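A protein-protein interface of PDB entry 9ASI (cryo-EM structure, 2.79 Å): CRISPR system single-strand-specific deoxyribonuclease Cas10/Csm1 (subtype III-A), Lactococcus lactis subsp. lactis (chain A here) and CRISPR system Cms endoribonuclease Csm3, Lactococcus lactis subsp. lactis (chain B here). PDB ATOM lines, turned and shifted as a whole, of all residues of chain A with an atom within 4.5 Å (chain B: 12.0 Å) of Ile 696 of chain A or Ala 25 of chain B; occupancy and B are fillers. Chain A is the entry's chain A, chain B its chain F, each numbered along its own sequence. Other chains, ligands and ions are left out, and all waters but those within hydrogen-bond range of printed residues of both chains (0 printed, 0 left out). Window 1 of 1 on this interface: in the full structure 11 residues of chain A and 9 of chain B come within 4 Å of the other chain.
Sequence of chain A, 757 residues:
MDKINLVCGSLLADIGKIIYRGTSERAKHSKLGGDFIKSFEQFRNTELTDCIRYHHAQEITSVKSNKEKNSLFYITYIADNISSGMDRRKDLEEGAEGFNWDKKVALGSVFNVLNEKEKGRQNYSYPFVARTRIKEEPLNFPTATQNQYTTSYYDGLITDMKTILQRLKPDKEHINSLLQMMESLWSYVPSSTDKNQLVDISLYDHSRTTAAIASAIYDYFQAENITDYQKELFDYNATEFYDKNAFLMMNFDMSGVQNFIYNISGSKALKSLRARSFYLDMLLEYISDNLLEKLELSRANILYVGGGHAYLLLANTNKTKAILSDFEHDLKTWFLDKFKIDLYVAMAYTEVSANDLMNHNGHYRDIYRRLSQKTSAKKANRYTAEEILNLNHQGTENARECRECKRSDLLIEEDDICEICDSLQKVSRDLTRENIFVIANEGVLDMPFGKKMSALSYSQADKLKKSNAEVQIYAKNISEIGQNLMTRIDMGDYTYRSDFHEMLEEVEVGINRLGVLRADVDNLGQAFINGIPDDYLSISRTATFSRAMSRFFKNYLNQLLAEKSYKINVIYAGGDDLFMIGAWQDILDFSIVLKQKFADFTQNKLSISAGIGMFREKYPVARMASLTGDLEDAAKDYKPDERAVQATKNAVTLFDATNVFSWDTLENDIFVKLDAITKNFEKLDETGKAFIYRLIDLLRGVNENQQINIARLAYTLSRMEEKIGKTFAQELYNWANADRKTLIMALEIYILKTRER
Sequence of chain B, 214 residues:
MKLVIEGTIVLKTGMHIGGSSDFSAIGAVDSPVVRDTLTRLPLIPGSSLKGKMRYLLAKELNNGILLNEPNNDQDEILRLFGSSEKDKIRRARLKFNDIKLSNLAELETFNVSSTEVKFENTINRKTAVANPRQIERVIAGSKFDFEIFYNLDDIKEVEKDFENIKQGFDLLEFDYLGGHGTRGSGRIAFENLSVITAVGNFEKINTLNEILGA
O of Ile 26 of chain B sits close to NH2 of Arg 755 of chain A (2.3 Å).
The backbone carbonyl oxygen (O) of Ala 28 of chain B sits close to the side-chain amide oxygen (OE1) of Gln 134 of chain B (2.8 Å).
N of Gln 134 of chain B is in hydrogen-bond range of OD2 of Asp 30 of chain B (2.5 Å).
OH of Tyr 693 of chain A sits at hydrogen-bond distance from OD2 of Asp 697 of chain A, 2.9 Å away.
The guanidinium group of Arg 700 of chain A is in salt-bridge range of the side-chain carboxylate of Asp 697 of chain A.
Ile 692 of chain A touches Ile 26 of chain B (CB to CD1, 3.6 Å).
Gly 27 of chain B touches Tyr 693 of chain A.
Tyr 693 of chain A touches Ala 28 of chain B.
Tyr 693 of chain A touches Val 29 of chain B (OH to CG1, 3.9 Å).
Gln 134 of chain B touches Tyr 693 of chain A.
Ile 696 of chain A touches Ala 25 of chain B (CD1 to CB, 3.6 Å).
Phe 23 of chain B touches Arg 700 of chain A (CE2 to CB, 3.9 Å).
Ala 25 of chain B touches Ile 751 of chain A.
Ile 751 of chain A touches Ile 26 of chain B (CG2 to N, 3.3 Å).
Ile 692 of chain A touches just one residue of chain B: Ile 26 (3.6 Å).
Of chain B, only Gly 27, Ala 28, Val 29 and Gln 134 come within 4 Å of Tyr 693 of chain A.
No residue of chain B comes within 4 Å of Leu 695 of chain A.
Of chain B, only Ala 25 comes within 4 Å of Ile 696 of chain A.
Leu 698 of chain A touches none of the printed residues of chain B.
Leu 699 of chain A touches none of the printed residues of chain B.
Printed residues of chain B within 4 Å of Arg 700 of chain A: Phe 23 (3.9 Å).
Ile 751 of chain A touches two residues of chain B.
Printed residues of chain B within 4 Å of Arg 755 of chain A: Ile 26.
Printed residues of chain A within 4 Å of Ile 26 of chain B: Ile 692, Ile 751 and Arg 755.
Of the printed residues of chain A, Ala 28 of chain B touches Tyr 693 (3.1 Å).
Printed residues of chain A within 4 Å of Val 29 of chain B: Tyr 693 (3.9 Å).
The nearest residue of chain A that does not touch Ala 25 of chain B is Tyr 693 of chain A (4.2 Å).
Of the 11 printed residues of chain A, 6 touch a printed residue of chain B.
Hydrophobic or aromatic side chains of chain A that line the printed part of chain B: Ile 692, Tyr 693, Ile 696 and Ile 751.
Of the 21 printed residues of chain B, 7 touch a printed residue of chain A.
Hydrophobic or aromatic side chains of chain B within 4 Å of the printed part of chain A: Phe 23, Ala 25, Ile 26 and Val 29.
Among the printed residues, 10 pairs touch across the chains.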
ATOM      1  N   ILE A 692     -34.464  10.773  -4.179  1.00  0.00           N
ATOM      2  CA  ILE A 692     -34.368  10.016  -2.934  1.00  0.00           C
ATOM      3  C   ILE A 692     -33.197   9.039  -2.983  1.00  0.00           C
ATOM      4  O   ILE A 692     -32.383   8.975  -2.054  1.00  0.00           O
ATOM      5  CB  ILE A 692     -35.696   9.297  -2.643  1.00  0.00           C
ATOM      6  CG1 ILE A 692     -36.812  10.317  -2.404  1.00  0.00           C
ATOM      7  CG2 ILE A 692     -35.550   8.378  -1.447  1.00  0.00           C
ATOM      8  CD1 ILE A 692     -38.173   9.696  -2.176  1.00  0.00           C
ATOM      9  N   TYR A 693     -33.091   8.263  -4.067  1.00  0.00           N
ATOM     10  CA  TYR A 693     -31.935   7.384  -4.217  1.00  0.00           C
ATOM     11  C   TYR A 693     -30.649   8.183  -4.379  1.00  0.00           C
ATOM     12  O   TYR A 693     -29.584   7.735  -3.946  1.00  0.00           O
ATOM     13  CB  TYR A 693     -32.125   6.441  -5.405  1.00  0.00           C
ATOM     14  CG  TYR A 693     -30.846   5.764  -5.861  1.00  0.00           C
ATOM     15  CD1 TYR A 693     -30.059   5.037  -4.970  1.00  0.00           C
ATOM     16  CD2 TYR A 693     -30.423   5.850  -7.183  1.00  0.00           C
ATOM     17  CE1 TYR A 693     -28.889   4.425  -5.381  1.00  0.00           C
ATOM     18  CE2 TYR A 693     -29.255   5.236  -7.603  1.00  0.00           C
ATOM     19  CZ  TYR A 693     -28.494   4.525  -6.698  1.00  0.00           C
ATOM     20  OH  TYR A 693     -27.333   3.914  -7.107  1.00  0.00           O
ATOM     21  N   ARG A 694     -30.727   9.358  -5.002  1.00  0.00           N
ATOM     22  CA  ARG A 694     -29.569  10.240  -5.072  1.00  0.00           C
ATOM     23  C   ARG A 694     -29.046  10.552  -3.675  1.00  0.00           C
ATOM     24  O   ARG A 694     -27.858  10.369  -3.381  1.00  0.00           O
ATOM     25  CB  ARG A 694     -29.960  11.519  -5.812  1.00  0.00           C
ATOM     26  CG  ARG A 694     -28.837  12.474  -6.137  1.00  0.00           C
ATOM     27  CD  ARG A 694     -29.308  13.426  -7.224  1.00  0.00           C
ATOM     28  NE  ARG A 694     -30.396  14.274  -6.754  1.00  0.00           N
ATOM     29  CZ  ARG A 694     -30.382  15.598  -6.786  1.00  0.00           C
ATOM     30  NH1 ARG A 694     -29.369  16.265  -7.310  1.00  0.00           N
ATOM     31  NH2 ARG A 694     -31.415  16.272  -6.287  1.00  0.00           N
ATOM     32  N   LEU A 695     -29.946  10.985  -2.788  1.00  0.00           N
ATOM     33  CA  LEU A 695     -29.568  11.260  -1.407  1.00  0.00           C
ATOM     34  C   LEU A 695     -29.037  10.010  -0.720  1.00  0.00           C
ATOM     35  O   LEU A 695     -28.036  10.069   0.004  1.00  0.00           O
ATOM     36  CB  LEU A 695     -30.768  11.815  -0.638  1.00  0.00           C
ATOM     37  CG  LEU A 695     -31.340  13.155  -1.097  1.00  0.00           C
ATOM     38  CD1 LEU A 695     -32.655  13.441  -0.390  1.00  0.00           C
ATOM     39  CD2 LEU A 695     -30.344  14.275  -0.854  1.00  0.00           C
ATOM     40  N   ILE A 696     -29.690   8.866  -0.938  1.00  0.00           N
ATOM     41  CA  ILE A 696     -29.307   7.642  -0.237  1.00  0.00           C
ATOM     42  C   ILE A 696     -27.900   7.210  -0.634  1.00  0.00           C
ATOM     43  O   ILE A 696     -27.055   6.919   0.221  1.00  0.00           O
ATOM     44  CB  ILE A 696     -30.338   6.529  -0.500  1.00  0.00           C
ATOM     45  CG1 ILE A 696     -31.620   6.803   0.287  1.00  0.00           C
ATOM     46  CG2 ILE A 696     -29.764   5.170  -0.133  1.00  0.00           C
ATOM     47  CD1 ILE A 696     -32.740   5.840  -0.014  1.00  0.00           C
ATOM     48  N   ASP A 697     -27.620   7.174  -1.937  1.00  0.00           N
ATOM     49  CA  ASP A 697     -26.317   6.726  -2.404  1.00  0.00           C
ATOM     50  C   ASP A 697     -25.229   7.772  -2.221  1.00  0.00           C
ATOM     51  O   ASP A 697     -24.045   7.419  -2.254  1.00  0.00           O
ATOM     52  CB  ASP A 697     -26.384   6.317  -3.876  1.00  0.00           C
ATOM     53  CG  ASP A 697     -25.320   5.296  -4.247  1.00  0.00           C
ATOM     54  OD1 ASP A 697     -24.582   4.854  -3.342  1.00  0.00           O
ATOM     55  OD2 ASP A 697     -25.220   4.937  -5.440  1.00  0.00           O
ATOM     56  N   LEU A 698     -25.584   9.044  -2.038  1.00  0.00           N
ATOM     57  CA  LEU A 698     -24.563  10.032  -1.722  1.00  0.00           C
ATOM     58  C   LEU A 698     -24.379  10.247  -0.225  1.00  0.00           C
ATOM     59  O   LEU A 698     -23.443  10.948   0.172  1.00  0.00           O
ATOM     60  CB  LEU A 698     -24.876  11.367  -2.403  1.00  0.00           C
ATOM     61  CG  LEU A 698     -24.313  11.479  -3.822  1.00  0.00           C
ATOM     62  CD1 LEU A 698     -22.800  11.335  -3.766  1.00  0.00           C
ATOM     63  CD2 LEU A 698     -24.919  10.468  -4.785  1.00  0.00           C
ATOM     64  N   LEU A 699     -25.241   9.668   0.607  1.00  0.00           N
ATOM     65  CA  LEU A 699     -25.083   9.734   2.051  1.00  0.00           C
ATOM     66  C   LEU A 699     -24.764   8.371   2.653  1.00  0.00           C
ATOM     67  O   LEU A 699     -24.581   8.273   3.871  1.00  0.00           O
ATOM     68  CB  LEU A 699     -26.350  10.344   2.674  1.00  0.00           C
ATOM     69  CG  LEU A 699     -26.438  10.849   4.119  1.00  0.00           C
ATOM     70  CD1 LEU A 699     -27.440  11.983   4.168  1.00  0.00           C
ATOM     71  CD2 LEU A 699     -26.867   9.771   5.095  1.00  0.00           C
ATOM     72  N   ARG A 700     -24.666   7.325   1.825  1.00  0.00           N
ATOM     73  CA  ARG A 700     -24.246   5.990   2.250  1.00  0.00           C
ATOM     74  C   ARG A 700     -23.070   6.026   3.222  1.00  0.00           C
ATOM     75  O   ARG A 700     -22.986   5.198   4.135  1.00  0.00           O
ATOM     76  CB  ARG A 700     -23.889   5.136   1.029  1.00  0.00           C
ATOM     77  CG  ARG A 700     -22.744   5.682   0.180  1.00  0.00           C
ATOM     78  CD  ARG A 700     -22.346   4.700  -0.914  1.00  0.00           C
ATOM     79  NE  ARG A 700     -21.499   5.313  -1.932  1.00  0.00           N
ATOM     80  CZ  ARG A 700     -20.177   5.389  -1.863  1.00  0.00           C
ATOM     81  NH1 ARG A 700     -19.509   4.905  -0.828  1.00  0.00           N
ATOM     82  NH2 ARG A 700     -19.507   5.963  -2.858  1.00  0.00           N
ATOM     83  N   ILE A 751     -37.953   3.545   2.961  1.00  0.00           N
ATOM     84  CA  ILE A 751     -37.883   3.015   1.601  1.00  0.00           C
ATOM     85  C   ILE A 751     -38.346   1.567   1.567  1.00  0.00           C
ATOM     86  O   ILE A 751     -39.151   1.175   0.713  1.00  0.00           O
ATOM     87  CB  ILE A 751     -36.457   3.164   1.041  1.00  0.00           C
ATOM     88  CG1 ILE A 751     -36.083   4.643   0.909  1.00  0.00           C
ATOM     89  CG2 ILE A 751     -36.305   2.411  -0.268  1.00  0.00           C
ATOM     90  CD1 ILE A 751     -37.009   5.428   0.012  1.00  0.00           C
ATOM     91  N   ARG A 755     -41.521   0.596  -0.562  1.00  0.00           N
ATOM     92  CA  ARG A 755     -41.038   0.185  -1.873  1.00  0.00           C
ATOM     93  C   ARG A 755     -42.116  -0.610  -2.601  1.00  0.00           C
ATOM     94  O   ARG A 755     -42.692  -1.551  -2.048  1.00  0.00           O
ATOM     95  CB  ARG A 755     -39.759  -0.643  -1.745  1.00  0.00           C
ATOM     96  CG  ARG A 755     -39.099  -0.981  -3.079  1.00  0.00           C
ATOM     97  CD  ARG A 755     -39.197   0.193  -4.045  1.00  0.00           C
ATOM     98  NE  ARG A 755     -38.283   0.085  -5.175  1.00  0.00           N
ATOM     99  CZ  ARG A 755     -38.375   0.818  -6.277  1.00  0.00           C
ATOM    100  NH1 ARG A 755     -39.353   1.691  -6.447  1.00  0.00           N
ATOM    101  NH2 ARG A 755     -37.458   0.676  -7.228  1.00  0.00           N
ATOM    102  N   SER B  20     -24.906  -9.838  -4.189  1.00  0.00           N
ATOM    103  CA  SER B  20     -24.843  -9.722  -2.736  1.00  0.00           C
ATOM    104  C   SER B  20     -26.035  -8.875  -2.304  1.00  0.00           C
ATOM    105  O   SER B  20     -26.023  -7.650  -2.450  1.00  0.00           O
ATOM    106  CB  SER B  20     -23.518  -9.108  -2.293  1.00  0.00           C
ATOM    107  OG  SER B  20     -23.330  -7.828  -2.870  1.00  0.00           O
ATOM    108  N   SER B  21     -27.062  -9.532  -1.770  1.00  0.00           N
ATOM    109  CA  SER B  21     -28.338  -8.881  -1.476  1.00  0.00           C
ATOM    110  C   SER B  21     -28.231  -8.123  -0.159  1.00  0.00           C
ATOM    111  O   SER B  21     -28.286  -8.717   0.920  1.00  0.00           O
ATOM    112  CB  SER B  21     -29.460  -9.911  -1.425  1.00  0.00           C
ATOM    113  OG  SER B  21     -29.291 -10.790  -0.325  1.00  0.00           O
ATOM    114  N   ASP B  22     -28.087  -6.801  -0.249  1.00  0.00           N
ATOM    115  CA  ASP B  22     -28.069  -5.924   0.915  1.00  0.00           C
ATOM    116  C   ASP B  22     -28.101  -4.476   0.446  1.00  0.00           C
ATOM    117  O   ASP B  22     -27.650  -4.161  -0.660  1.00  0.00           O
ATOM    118  CB  ASP B  22     -26.831  -6.162   1.795  1.00  0.00           C
ATOM    119  CG  ASP B  22     -25.532  -6.038   1.024  1.00  0.00           C
ATOM    120  OD1 ASP B  22     -25.569  -6.060  -0.224  1.00  0.00           O
ATOM    121  OD2 ASP B  22     -24.470  -5.915   1.669  1.00  0.00           O
ATOM    122  N   PHE B  23     -28.643  -3.606   1.302  1.00  0.00           N
ATOM    123  CA  PHE B  23     -28.577  -2.153   1.139  1.00  0.00           C
ATOM    124  C   PHE B  23     -29.149  -1.715  -0.215  1.00  0.00           C
ATOM    125  O   PHE B  23     -28.449  -1.203  -1.091  1.00  0.00           O
ATOM    126  CB  PHE B  23     -27.138  -1.656   1.320  1.00  0.00           C
ATOM    127  CG  PHE B  23     -27.042  -0.200   1.680  1.00  0.00           C
ATOM    128  CD1 PHE B  23     -27.623   0.277   2.843  1.00  0.00           C
ATOM    129  CD2 PHE B  23     -26.371   0.689   0.857  1.00  0.00           C
ATOM    130  CE1 PHE B  23     -27.537   1.614   3.177  1.00  0.00           C
ATOM    131  CE2 PHE B  23     -26.283   2.028   1.187  1.00  0.00           C
ATOM    132  CZ  PHE B  23     -26.866   2.491   2.347  1.00  0.00           C
ATOM    133  N   SER B  24     -30.453  -1.936  -0.361  1.00  0.00           N
ATOM    134  CA  SER B  24     -31.186  -1.555  -1.560  1.00  0.00           C
ATOM    135  C   SER B  24     -32.154  -0.421  -1.247  1.00  0.00           C
ATOM    136  O   SER B  24     -32.789  -0.406  -0.188  1.00  0.00           O
ATOM    137  CB  SER B  24     -31.949  -2.749  -2.141  1.00  0.00           C
ATOM    138  OG  SER B  24     -33.020  -3.132  -1.295  1.00  0.00           O
ATOM    139  N   ALA B  25     -32.255   0.530  -2.172  1.00  0.00           N
ATOM    140  CA  ALA B  25     -33.146   1.676  -2.094  1.00  0.00           C
ATOM    141  C   ALA B  25     -34.198   1.587  -3.202  1.00  0.00           C
ATOM    142  O   ALA B  25     -34.296   0.581  -3.913  1.00  0.00           O
ATOM    143  CB  ALA B  25     -32.339   2.971  -2.180  1.00  0.00           C
ATOM    144  N   ILE B  26     -35.005   2.642  -3.343  1.00  0.00           N
ATOM    145  CA  ILE B  26     -35.993   2.664  -4.419  1.00  0.00           C
ATOM    146  C   ILE B  26     -35.299   2.728  -5.776  1.00  0.00           C
ATOM    147  O   ILE B  26     -35.606   1.948  -6.685  1.00  0.00           O
ATOM    148  CB  ILE B  26     -36.987   3.826  -4.234  1.00  0.00           C
ATOM    149  CG1 ILE B  26     -36.259   5.138  -3.937  1.00  0.00           C
ATOM    150  CG2 ILE B  26     -38.000   3.505  -3.147  1.00  0.00           C
ATOM    151  CD1 ILE B  26     -37.116   6.358  -4.168  1.00  0.00           C
ATOM    152  N   GLY B  27     -34.355   3.652  -5.937  1.00  0.00           N
ATOM    153  CA  GLY B  27     -33.526   3.650  -7.123  1.00  0.00           C
ATOM    154  C   GLY B  27     -32.532   2.512  -7.065  1.00  0.00           C
ATOM    155  O   GLY B  27     -32.637   1.540  -7.821  1.00  0.00           O
ATOM    156  N   ALA B  28     -31.569   2.628  -6.150  1.00  0.00           N
ATOM    157  CA  ALA B  28     -30.638   1.560  -5.802  1.00  0.00           C
ATOM    158  C   ALA B  28     -29.793   1.082  -6.972  1.00  0.00           C
ATOM    159  O   ALA B  28     -29.970   1.521  -8.112  1.00  0.00           O
ATOM    160  CB  ALA B  28     -31.395   0.368  -5.215  1.00  0.00           C
ATOM    161  N   VAL B  29     -28.843   0.201  -6.684  1.00  0.00           N
ATOM    162  CA  VAL B  29     -28.339  -0.736  -7.674  1.00  0.00           C
ATOM    163  C   VAL B  29     -29.152  -2.013  -7.494  1.00  0.00           C
ATOM    164  O   VAL B  29     -29.023  -2.719  -6.491  1.00  0.00           O
ATOM    165  CB  VAL B  29     -26.828  -0.966  -7.543  1.00  0.00           C
ATOM    166  CG1 VAL B  29     -26.093   0.310  -7.878  1.00  0.00           C
ATOM    167  CG2 VAL B  29     -26.441  -1.393  -6.130  1.00  0.00           C
ATOM    168  N   ASP B  30     -30.048  -2.274  -8.445  1.00  0.00           N
ATOM    169  CA  ASP B  30     -30.962  -3.398  -8.306  1.00  0.00           C
ATOM    170  C   ASP B  30     -30.225  -4.726  -8.254  1.00  0.00           C
ATOM    171  O   ASP B  30     -30.762  -5.702  -7.721  1.00  0.00           O
ATOM    172  CB  ASP B  30     -31.969  -3.381  -9.453  1.00  0.00           C
ATOM    173  CG  ASP B  30     -32.772  -2.096  -9.504  1.00  0.00           C
ATOM    174  OD1 ASP B  30     -33.583  -1.864  -8.584  1.00  0.00           O
ATOM    175  OD2 ASP B  30     -32.592  -1.318 -10.460  1.00  0.00           O
ATOM    176  N   SER B  31     -29.010  -4.781  -8.788  1.00  0.00           N
ATOM    177  CA  SER B  31     -28.156  -5.949  -8.660  1.00  0.00           C
ATOM    178  C   SER B  31     -26.712  -5.492  -8.508  1.00  0.00           C
ATOM    179  O   SER B  31     -26.116  -4.989  -9.469  1.00  0.00           O
ATOM    180  CB  SER B  31     -28.304  -6.871  -9.869  1.00  0.00           C
ATOM    181  OG  SER B  31     -27.621  -6.349 -10.991  1.00  0.00           O
ATOM    182  N   PRO B  32     -26.119  -5.641  -7.331  1.00  0.00           N
ATOM    183  CA  PRO B  32     -24.723  -5.252  -7.133  1.00  0.00           C
ATOM    184  C   PRO B  32     -23.788  -6.360  -7.603  1.00  0.00           C
ATOM    185  O   PRO B  32     -24.212  -7.435  -8.013  1.00  0.00           O
ATOM    186  CB  PRO B  32     -24.625  -5.033  -5.620  1.00  0.00           C
ATOM    187  CG  PRO B  32     -25.891  -5.608  -5.028  1.00  0.00           C
ATOM    188  CD  PRO B  32     -26.700  -6.227  -6.115  1.00  0.00           C
ATOM    189  N   VAL B 117     -22.829   2.298 -12.445  1.00  0.00           N
ATOM    190  CA  VAL B 117     -24.234   1.923 -12.357  1.00  0.00           C
ATOM    191  C   VAL B 117     -24.823   2.057 -13.752  1.00  0.00           C
ATOM    192  O   VAL B 117     -24.985   3.172 -14.262  1.00  0.00           O
ATOM    193  CB  VAL B 117     -24.999   2.786 -11.348  1.00  0.00           C
ATOM    194  CG1 VAL B 117     -26.456   2.371 -11.303  1.00  0.00           C
ATOM    195  CG2 VAL B 117     -24.368   2.674  -9.975  1.00  0.00           C
ATOM    196  N   PHE B 119     -27.805   1.956 -16.346  1.00  0.00           N
ATOM    197  CA  PHE B 119     -29.244   2.168 -16.358  1.00  0.00           C
ATOM    198  C   PHE B 119     -29.836   1.445 -17.558  1.00  0.00           C
ATOM    199  O   PHE B 119     -29.411   1.667 -18.696  1.00  0.00           O
ATOM    200  CB  PHE B 119     -29.577   3.657 -16.404  1.00  0.00           C
ATOM    201  CG  PHE B 119     -29.312   4.375 -15.116  1.00  0.00           C
ATOM    202  CD1 PHE B 119     -28.024   4.733 -14.762  1.00  0.00           C
ATOM    203  CD2 PHE B 119     -30.350   4.697 -14.262  1.00  0.00           C
ATOM    204  CE1 PHE B 119     -27.777   5.393 -13.581  1.00  0.00           C
ATOM    205  CE2 PHE B 119     -30.109   5.358 -13.080  1.00  0.00           C
ATOM    206  CZ  PHE B 119     -28.819   5.706 -12.738  1.00  0.00           C
ATOM    207  N   ASN B 131     -39.650   0.082 -17.864  1.00  0.00           N
ATOM    208  CA  ASN B 131     -39.366  -0.356 -16.502  1.00  0.00           C
ATOM    209  C   ASN B 131     -37.874  -0.217 -16.214  1.00  0.00           C
ATOM    210  O   ASN B 131     -37.090  -1.093 -16.593  1.00  0.00           O
ATOM    211  CB  ASN B 131     -39.831  -1.800 -16.309  1.00  0.00           C
ATOM    212  CG  ASN B 131     -39.860  -2.219 -14.855  1.00  0.00           C
ATOM    213  OD1 ASN B 131     -39.477  -1.462 -13.969  1.00  0.00           O
ATOM    214  ND2 ASN B 131     -40.318  -3.438 -14.603  1.00  0.00           N
ATOM    215  N   PRO B 132     -37.446   0.844 -15.527  1.00  0.00           N
ATOM    216  CA  PRO B 132     -36.018   1.181 -15.453  1.00  0.00           C
ATOM    217  C   PRO B 132     -35.283   0.378 -14.391  1.00  0.00           C
ATOM    218  O   PRO B 132     -35.405   0.656 -13.195  1.00  0.00           O
ATOM    219  CB  PRO B 132     -36.041   2.674 -15.105  1.00  0.00           C
ATOM    220  CG  PRO B 132     -37.359   2.877 -14.391  1.00  0.00           C
ATOM    221  CD  PRO B 132     -38.247   1.688 -14.629  1.00  0.00           C
ATOM    222  N   ARG B 133     -34.451  -0.562 -14.823  1.00  0.00           N
ATOM    223  CA  ARG B 133     -33.616  -1.310 -13.895  1.00  0.00           C
ATOM    224  C   ARG B 133     -32.197  -0.753 -13.879  1.00  0.00           C
ATOM    225  O   ARG B 133     -31.690  -0.269 -14.892  1.00  0.00           O
ATOM    226  CB  ARG B 133     -33.584  -2.797 -14.249  1.00  0.00           C
ATOM    227  CG  ARG B 133     -33.179  -3.096 -15.670  1.00  0.00           C
ATOM    228  CD  ARG B 133     -33.987  -4.245 -16.239  1.00  0.00           C
ATOM    229  NE  ARG B 133     -33.734  -4.440 -17.661  1.00  0.00           N
ATOM    230  CZ  ARG B 133     -32.626  -4.970 -18.155  1.00  0.00           C
ATOM    231  NH1 ARG B 133     -31.640  -5.365 -17.370  1.00  0.00           N
ATOM    232  NH2 ARG B 133     -32.507  -5.113 -19.470  1.00  0.00           N
ATOM    233  N   GLN B 134     -31.562  -0.821 -12.714  1.00  0.00           N
ATOM    234  CA  GLN B 134     -30.184  -0.383 -12.538  1.00  0.00           C
ATOM    235  C   GLN B 134     -29.308  -1.585 -12.222  1.00  0.00           C
ATOM    236  O   GLN B 134     -29.633  -2.376 -11.332  1.00  0.00           O
ATOM    237  CB  GLN B 134     -30.072   0.649 -11.418  1.00  0.00           C
ATOM    238  CG  GLN B 134     -31.116   1.733 -11.469  1.00  0.00           C
ATOM    239  CD  GLN B 134     -30.701   2.965 -10.706  1.00  0.00           C
ATOM    240  OE1 GLN B 134     -29.525   3.149 -10.396  1.00  0.00           O
ATOM    241  NE2 GLN B 134     -31.664   3.820 -10.392  1.00  0.00           N
ATOM    242  N   ILE B 135     -28.201  -1.717 -12.945  1.00  0.00           N
ATOM    243  CA  ILE B 135     -27.286  -2.838 -12.789  1.00  0.00           C
ATOM    244  C   ILE B 135     -25.915  -2.273 -12.453  1.00  0.00           C
ATOM    245  O   ILE B 135     -25.267  -1.652 -13.305  1.00  0.00           O
ATOM    246  CB  ILE B 135     -27.221  -3.717 -14.046  1.00  0.00           C
ATOM    247  CG1 ILE B 135     -28.603  -4.254 -14.408  1.00  0.00           C
ATOM    248  CG2 ILE B 135     -26.267  -4.870 -13.836  1.00  0.00           C
ATOM    249  CD1 ILE B 135     -29.314  -3.444 -15.456  1.00  0.00           C
ATOM    250  N   GLU B 136     -25.474  -2.482 -11.217  1.00  0.00           N
ATOM    251  CA  GLU B 136     -24.104  -2.156 -10.851  1.00  0.00           C
ATOM    252  C   GLU B 136     -23.146  -2.984 -11.694  1.00  0.00           C
ATOM    253  O   GLU B 136     -23.365  -4.174 -11.919  1.00  0.00           O
ATOM    254  CB  GLU B 136     -23.882  -2.424  -9.364  1.00  0.00           C
ATOM    255  CG  GLU B 136     -22.435  -2.386  -8.906  1.00  0.00           C
ATOM    256  CD  GLU B 136     -22.035  -1.044  -8.335  1.00  0.00           C
ATOM    257  OE1 GLU B 136     -22.843  -0.096  -8.410  1.00  0.00           O
ATOM    258  OE2 GLU B 136     -20.919  -0.939  -7.790  1.00  0.00           O
